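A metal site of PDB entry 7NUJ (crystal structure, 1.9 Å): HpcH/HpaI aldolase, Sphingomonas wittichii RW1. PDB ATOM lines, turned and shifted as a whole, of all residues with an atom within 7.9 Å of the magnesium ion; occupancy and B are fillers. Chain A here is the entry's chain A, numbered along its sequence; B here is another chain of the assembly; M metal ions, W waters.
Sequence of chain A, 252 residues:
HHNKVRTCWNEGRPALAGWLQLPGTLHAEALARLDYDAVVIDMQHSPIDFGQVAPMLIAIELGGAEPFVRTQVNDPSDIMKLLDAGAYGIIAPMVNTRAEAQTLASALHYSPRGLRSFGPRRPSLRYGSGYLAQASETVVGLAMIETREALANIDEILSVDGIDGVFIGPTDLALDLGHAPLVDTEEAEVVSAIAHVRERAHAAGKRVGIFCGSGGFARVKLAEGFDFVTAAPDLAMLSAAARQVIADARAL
Water W2 bridges the side-chain carboxylate of Asp 172 (3.4 Å) and the side-chain sulfur of Met 94 (3.8 Å). Water W1 bridges the side-chain carboxylate of Glu 146 (2.6 Å) and the side-chain amide nitrogen of Gln 44 (2.7 Å). Water W3 lies within hydrogen-bond range of the side-chain amide oxygen of Gln 44 and the guanidinium group of Arg 70.
Residues that only touch the magnesium ion: Gln 44 (3.9 Å). Within 4 Å of the magnesium ion: Gln 44, Glu 146, Asp 172 and Ser 117 of chain B. The nearest printed residue that does not touch the magnesium ion is His 45 (4.2 Å).
OG of Ser 117 of chain B sits close to NE2 of Gln 44 (3.4 Å). The side-chain hydroxyl (OG) of Ser 117 of chain B lies close to a ring nitrogen (NE2) of His 45, 2.7 Å away. N of Ser 117 of chain B sits at hydrogen-bond distance from SD of Met 80 of chain B, 3.5 Å away. The side-chain carboxylate (OE2) of Glu 146 lies within hydrogen-bond range of the backbone NH (N) of Met 94. The side-chain carboxylate (OD1) of Asp 172 is in hydrogen-bond range of the backbone NH (N) of Phe 118 of chain B (2.9 Å). The guanidinium group (NE) of Arg 70 sits close to the side-chain amide oxygen (OE1) of Gln 44 (3.1 Å).
The magnesium ion is bound by the side-chain hydroxyl of Ser 117 of chain B (2.0 Å), water W3 (2.0 Å), the side-chain carboxylate of Glu 146 (2.1 Å), the side-chain carboxylate of Asp 172 (2.1 Å), water W1 (2.1 Å) and water W2 (2.1 Å). The magnesium ion has six donor atoms within binding distance.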
ATOM      1  N   GLN A  44      -9.956 -18.779  -3.477  1.00  0.00           N
ATOM      2  CA  GLN A  44      -9.550 -17.379  -3.204  1.00  0.00           C
ATOM      3  C   GLN A  44     -10.634 -16.413  -3.692  1.00  0.00           C
ATOM      4  O   GLN A  44     -11.238 -15.743  -2.846  1.00  0.00           O
ATOM      5  CB  GLN A  44      -8.195 -17.118  -3.848  1.00  0.00           C
ATOM      6  CG  GLN A  44      -7.657 -15.719  -3.575  1.00  0.00           C
ATOM      7  CD  GLN A  44      -6.327 -15.518  -4.246  1.00  0.00           C
ATOM      8  OE1 GLN A  44      -6.093 -15.947  -5.376  1.00  0.00           O
ATOM      9  NE2 GLN A  44      -5.430 -14.865  -3.534  1.00  0.00           N
ATOM     10  N   HIS A  45     -10.834 -16.305  -5.007  1.00  0.00           N
ATOM     11  CA  HIS A  45     -11.734 -15.311  -5.668  1.00  0.00           C
ATOM     12  C   HIS A  45     -13.063 -15.979  -6.010  1.00  0.00           C
ATOM     13  O   HIS A  45     -13.415 -16.080  -7.168  1.00  0.00           O
ATOM     14  CB  HIS A  45     -11.000 -14.630  -6.819  1.00  0.00           C
ATOM     15  CG  HIS A  45      -9.868 -13.804  -6.325  1.00  0.00           C
ATOM     16  ND1 HIS A  45     -10.074 -12.721  -5.483  1.00  0.00           N
ATOM     17  CD2 HIS A  45      -8.535 -13.885  -6.531  1.00  0.00           C
ATOM     18  CE1 HIS A  45      -8.901 -12.193  -5.182  1.00  0.00           C
ATOM     19  NE2 HIS A  45      -7.943 -12.879  -5.817  1.00  0.00           N
ATOM     20  N   ARG A  70      -6.847 -23.911  -6.133  1.00  0.00           N
ATOM     21  CA  ARG A  70      -6.126 -22.659  -5.922  1.00  0.00           C
ATOM     22  C   ARG A  70      -6.542 -22.175  -4.529  1.00  0.00           C
ATOM     23  O   ARG A  70      -7.668 -21.757  -4.371  1.00  0.00           O
ATOM     24  CB  ARG A  70      -6.345 -21.643  -7.047  1.00  0.00           C
ATOM     25  CG  ARG A  70      -5.400 -20.460  -6.975  1.00  0.00           C
ATOM     26  CD  ARG A  70      -5.928 -19.273  -6.202  1.00  0.00           C
ATOM     27  NE  ARG A  70      -6.960 -18.542  -6.935  1.00  0.00           N
ATOM     28  CZ  ARG A  70      -6.760 -17.641  -7.915  1.00  0.00           C
ATOM     29  NH1 ARG A  70      -5.544 -17.323  -8.337  1.00  0.00           N
ATOM     30  NH2 ARG A  70      -7.814 -17.056  -8.497  1.00  0.00           N
ATOM     31  N   GLN A  72      -6.727 -20.029  -0.845  1.00  0.00           N
ATOM     32  CA  GLN A  72      -6.860 -18.626  -0.388  1.00  0.00           C
ATOM     33  C   GLN A  72      -5.469 -18.075  -0.066  1.00  0.00           C
ATOM     34  O   GLN A  72      -5.264 -16.863  -0.222  1.00  0.00           O
ATOM     35  CB  GLN A  72      -7.763 -18.671   0.834  1.00  0.00           C
ATOM     36  CG  GLN A  72      -7.959 -17.351   1.512  1.00  0.00           C
ATOM     37  CD  GLN A  72      -8.703 -17.556   2.796  1.00  0.00           C
ATOM     38  OE1 GLN A  72      -9.770 -18.180   2.815  1.00  0.00           O
ATOM     39  NE2 GLN A  72      -8.155 -16.974   3.851  1.00  0.00           N
ATOM     40  N   PRO A  93      -1.281 -18.942  -3.699  1.00  0.00           N
ATOM     41  CA  PRO A  93      -1.060 -17.543  -4.050  1.00  0.00           C
ATOM     42  C   PRO A  93       0.138 -16.901  -3.337  1.00  0.00           C
ATOM     43  O   PRO A  93       0.596 -17.371  -2.325  1.00  0.00           O
ATOM     44  CB  PRO A  93      -2.378 -16.854  -3.667  1.00  0.00           C
ATOM     45  CG  PRO A  93      -2.915 -17.703  -2.558  1.00  0.00           C
ATOM     46  CD  PRO A  93      -2.471 -19.122  -2.860  1.00  0.00           C
ATOM     47  N   MET A  94       0.614 -15.796  -3.909  1.00  0.00           N
ATOM     48  CA  MET A  94       1.549 -14.827  -3.283  1.00  0.00           C
ATOM     49  C   MET A  94       2.803 -15.547  -2.814  1.00  0.00           C
ATOM     50  O   MET A  94       3.222 -15.353  -1.675  1.00  0.00           O
ATOM     51  CB  MET A  94       0.848 -14.093  -2.128  1.00  0.00           C
ATOM     52  CG  MET A  94      -0.197 -13.129  -2.593  1.00  0.00           C
ATOM     53  SD  MET A  94       0.550 -11.800  -3.576  1.00  0.00           S
ATOM     54  CE  MET A  94       1.056 -10.673  -2.273  1.00  0.00           C
ATOM     55  N   MET A 144       2.314 -19.563  -7.089  1.00  0.00           N
ATOM     56  CA  MET A 144       1.848 -18.427  -7.921  1.00  0.00           C
ATOM     57  C   MET A 144       2.906 -17.330  -7.999  1.00  0.00           C
ATOM     58  O   MET A 144       3.492 -16.971  -6.960  1.00  0.00           O
ATOM     59  CB  MET A 144       0.551 -17.812  -7.410  1.00  0.00           C
ATOM     60  CG  MET A 144      -0.658 -18.671  -7.750  1.00  0.00           C
ATOM     61  SD  MET A 144      -2.184 -17.800  -7.449  1.00  0.00           S
ATOM     62  CE  MET A 144      -2.253 -16.725  -8.891  1.00  0.00           C
ATOM     63  N   ILE A 145       3.078 -16.806  -9.208  1.00  0.00           N
ATOM     64  CA  ILE A 145       3.876 -15.608  -9.571  1.00  0.00           C
ATOM     65  C   ILE A 145       2.869 -14.527 -10.016  1.00  0.00           C
ATOM     66  O   ILE A 145       2.294 -14.650 -11.122  1.00  0.00           O
ATOM     67  CB  ILE A 145       4.907 -15.962 -10.659  1.00  0.00           C
ATOM     68  CG1 ILE A 145       5.755 -17.181 -10.245  1.00  0.00           C
ATOM     69  CG2 ILE A 145       5.747 -14.746 -11.044  1.00  0.00           C
ATOM     70  CD1 ILE A 145       6.666 -16.993  -9.036  1.00  0.00           C
ATOM     71  N   GLU A 146       2.633 -13.546  -9.152  1.00  0.00           N
ATOM     72  CA  GLU A 146       1.609 -12.492  -9.383  1.00  0.00           C
ATOM     73  C   GLU A 146       2.043 -11.144  -8.812  1.00  0.00           C
ATOM     74  O   GLU A 146       1.156 -10.267  -8.664  1.00  0.00           O
ATOM     75  CB  GLU A 146       0.275 -13.014  -8.860  1.00  0.00           C
ATOM     76  CG  GLU A 146       0.330 -13.636  -7.462  1.00  0.00           C
ATOM     77  CD  GLU A 146      -1.010 -13.855  -6.769  1.00  0.00           C
ATOM     78  OE1 GLU A 146      -1.978 -13.271  -7.195  1.00  0.00           O
ATOM     79  OE2 GLU A 146      -1.052 -14.563  -5.758  1.00  0.00           O
ATOM     80  N   THR A 147       3.340 -10.929  -8.556  1.00  0.00           N
ATOM     81  CA  THR A 147       3.894  -9.650  -8.050  1.00  0.00           C
ATOM     82  C   THR A 147       5.239  -9.371  -8.732  1.00  0.00           C
ATOM     83  O   THR A 147       5.931 -10.327  -9.181  1.00  0.00           O
ATOM     84  CB  THR A 147       4.096  -9.668  -6.518  1.00  0.00           C
ATOM     85  OG1 THR A 147       5.182 -10.534  -6.167  1.00  0.00           O
ATOM     86  CG2 THR A 147       2.855 -10.081  -5.775  1.00  0.00           C
ATOM     87  N   GLY A 169      -0.410 -15.770 -12.401  1.00  0.00           N
ATOM     88  CA  GLY A 169      -1.660 -15.024 -12.223  1.00  0.00           C
ATOM     89  C   GLY A 169      -1.535 -13.687 -12.954  1.00  0.00           C
ATOM     90  O   GLY A 169      -1.053 -12.715 -12.375  1.00  0.00           O
ATOM     91  N   THR A 171      -3.434 -11.242 -14.253  1.00  0.00           N
ATOM     92  CA  THR A 171      -4.258 -10.048 -13.927  1.00  0.00           C
ATOM     93  C   THR A 171      -3.647  -9.323 -12.721  1.00  0.00           C
ATOM     94  O   THR A 171      -3.456  -8.098 -12.788  1.00  0.00           O
ATOM     95  CB  THR A 171      -5.739 -10.396 -13.679  1.00  0.00           C
ATOM     96  OG1 THR A 171      -5.845 -11.223 -12.524  1.00  0.00           O
ATOM     97  CG2 THR A 171      -6.344 -11.123 -14.861  1.00  0.00           C
ATOM     98  N   ASP A 172      -3.312 -10.061 -11.671  1.00  0.00           N
ATOM     99  CA  ASP A 172      -2.612  -9.490 -10.491  1.00  0.00           C
ATOM    100  C   ASP A 172      -1.212  -9.033 -10.905  1.00  0.00           C
ATOM    101  O   ASP A 172      -0.750  -7.976 -10.382  1.00  0.00           O
ATOM    102  CB  ASP A 172      -2.532 -10.484  -9.329  1.00  0.00           C
ATOM    103  CG  ASP A 172      -3.711 -10.428  -8.375  1.00  0.00           C
ATOM    104  OD1 ASP A 172      -4.133  -9.285  -8.030  1.00  0.00           O
ATOM    105  OD2 ASP A 172      -4.224 -11.526  -7.987  1.00  0.00           O
ATOM    106  N   LEU A 173      -0.527  -9.790 -11.761  1.00  0.00           N
ATOM    107  CA  LEU A 173       0.824  -9.382 -12.212  1.00  0.00           C
ATOM    108  C   LEU A 173       0.728  -8.061 -13.010  1.00  0.00           C
ATOM    109  O   LEU A 173       1.545  -7.159 -12.759  1.00  0.00           O
ATOM    110  CB  LEU A 173       1.464 -10.516 -13.036  1.00  0.00           C
ATOM    111  CG  LEU A 173       2.914 -10.271 -13.444  1.00  0.00           C
ATOM    112  CD1 LEU A 173       3.803 -10.088 -12.230  1.00  0.00           C
ATOM    113  CD2 LEU A 173       3.405 -11.422 -14.310  1.00  0.00           C
ATOM    114  N   MET B  80      -9.629 -10.435   2.410  1.00  0.00           N
ATOM    115  CA  MET B  80      -9.761 -10.322   0.934  1.00  0.00           C
ATOM    116  C   MET B  80     -10.929 -11.201   0.451  1.00  0.00           C
ATOM    117  O   MET B  80     -11.750 -10.700  -0.328  1.00  0.00           O
ATOM    118  CB  MET B  80      -8.466 -10.711   0.236  1.00  0.00           C
ATOM    119  CG  MET B  80      -7.349  -9.697   0.429  1.00  0.00           C
ATOM    120  SD  MET B  80      -5.858 -10.335  -0.359  1.00  0.00           S
ATOM    121  CE  MET B  80      -4.588  -9.511   0.584  1.00  0.00           C
ATOM    122  N   LEU B 115      -1.904  -4.717  -1.003  1.00  0.00           N
ATOM    123  CA  LEU B 115      -1.599  -5.960  -1.760  1.00  0.00           C
ATOM    124  C   LEU B 115      -2.865  -6.798  -1.940  1.00  0.00           C
ATOM    125  O   LEU B 115      -2.723  -8.013  -2.188  1.00  0.00           O
ATOM    126  CB  LEU B 115      -0.444  -6.715  -1.090  1.00  0.00           C
ATOM    127  CG  LEU B 115      -0.459  -6.817   0.433  1.00  0.00           C
ATOM    128  CD1 LEU B 115      -1.556  -7.770   0.907  1.00  0.00           C
ATOM    129  CD2 LEU B 115       0.909  -7.236   0.940  1.00  0.00           C
ATOM    130  N   ARG B 116      -4.041  -6.173  -1.874  1.00  0.00           N
ATOM    131  CA  ARG B 116      -5.318  -6.877  -2.139  1.00  0.00           C
ATOM    132  C   ARG B 116      -5.194  -7.626  -3.483  1.00  0.00           C
ATOM    133  O   ARG B 116      -4.851  -6.999  -4.468  1.00  0.00           O
ATOM    134  CB  ARG B 116      -6.498  -5.899  -2.137  1.00  0.00           C
ATOM    135  CG  ARG B 116      -7.840  -6.618  -2.238  1.00  0.00           C
ATOM    136  CD  ARG B 116      -8.981  -5.623  -2.291  1.00  0.00           C
ATOM    137  NE  ARG B 116     -10.213  -6.285  -2.679  1.00  0.00           N
ATOM    138  CZ  ARG B 116     -11.350  -5.676  -2.992  1.00  0.00           C
ATOM    139  NH1 ARG B 116     -11.435  -4.353  -2.985  1.00  0.00           N
ATOM    140  NH2 ARG B 116     -12.417  -6.406  -3.314  1.00  0.00           N
ATOM    141  N   SER B 117      -5.459  -8.930  -3.487  1.00  0.00           N
ATOM    142  CA  SER B 117      -5.561  -9.774  -4.689  1.00  0.00           C
ATOM    143  C   SER B 117      -6.826  -9.398  -5.475  1.00  0.00           C
ATOM    144  O   SER B 117      -7.878  -9.116  -4.882  1.00  0.00           O
ATOM    145  CB  SER B 117      -5.559 -11.247  -4.318  1.00  0.00           C
ATOM    146  OG  SER B 117      -5.431 -12.059  -5.476  1.00  0.00           O
ATOM    147  N   PHE B 118      -6.723  -9.405  -6.809  1.00  0.00           N
ATOM    148  CA  PHE B 118      -7.771  -8.937  -7.739  1.00  0.00           C
ATOM    149  C   PHE B 118      -8.601 -10.135  -8.188  1.00  0.00           C
ATOM    150  O   PHE B 118      -8.066 -11.019  -8.840  1.00  0.00           O
ATOM    151  CB  PHE B 118      -7.175  -8.168  -8.919  1.00  0.00           C
ATOM    152  CG  PHE B 118      -8.242  -7.513  -9.755  1.00  0.00           C
ATOM    153  CD1 PHE B 118      -8.793  -6.297  -9.358  1.00  0.00           C
ATOM    154  CD2 PHE B 118      -8.769  -8.139 -10.869  1.00  0.00           C
ATOM    155  CE1 PHE B 118      -9.829  -5.704 -10.075  1.00  0.00           C
ATOM    156  CE2 PHE B 118      -9.815  -7.550 -11.588  1.00  0.00           C
ATOM    157  CZ  PHE B 118     -10.321  -6.333 -11.199  1.00  0.00           C
ATOM    158  N   GLY B 119      -9.880 -10.149  -7.818  1.00  0.00           N
ATOM    159  CA  GLY B 119     -10.937 -11.037  -8.339  1.00  0.00           C
ATOM    160  C   GLY B 119     -12.257 -10.723  -7.643  1.00  0.00           C
ATOM    161  O   GLY B 119     -12.774 -11.530  -6.879  1.00  0.00           O
HETATM  162 MG    MG M   1      -3.740 -12.646  -6.308  1.00  0.00          MG
HETATM  163  O   HOH W   1      -3.189 -13.662  -4.577  1.00  0.00           O
HETATM  164  O   HOH W   2      -2.571 -11.099  -5.547  1.00  0.00           O
HETATM  165  O   HOH W   3      -4.619 -14.325  -7.057  1.00  0.00           O
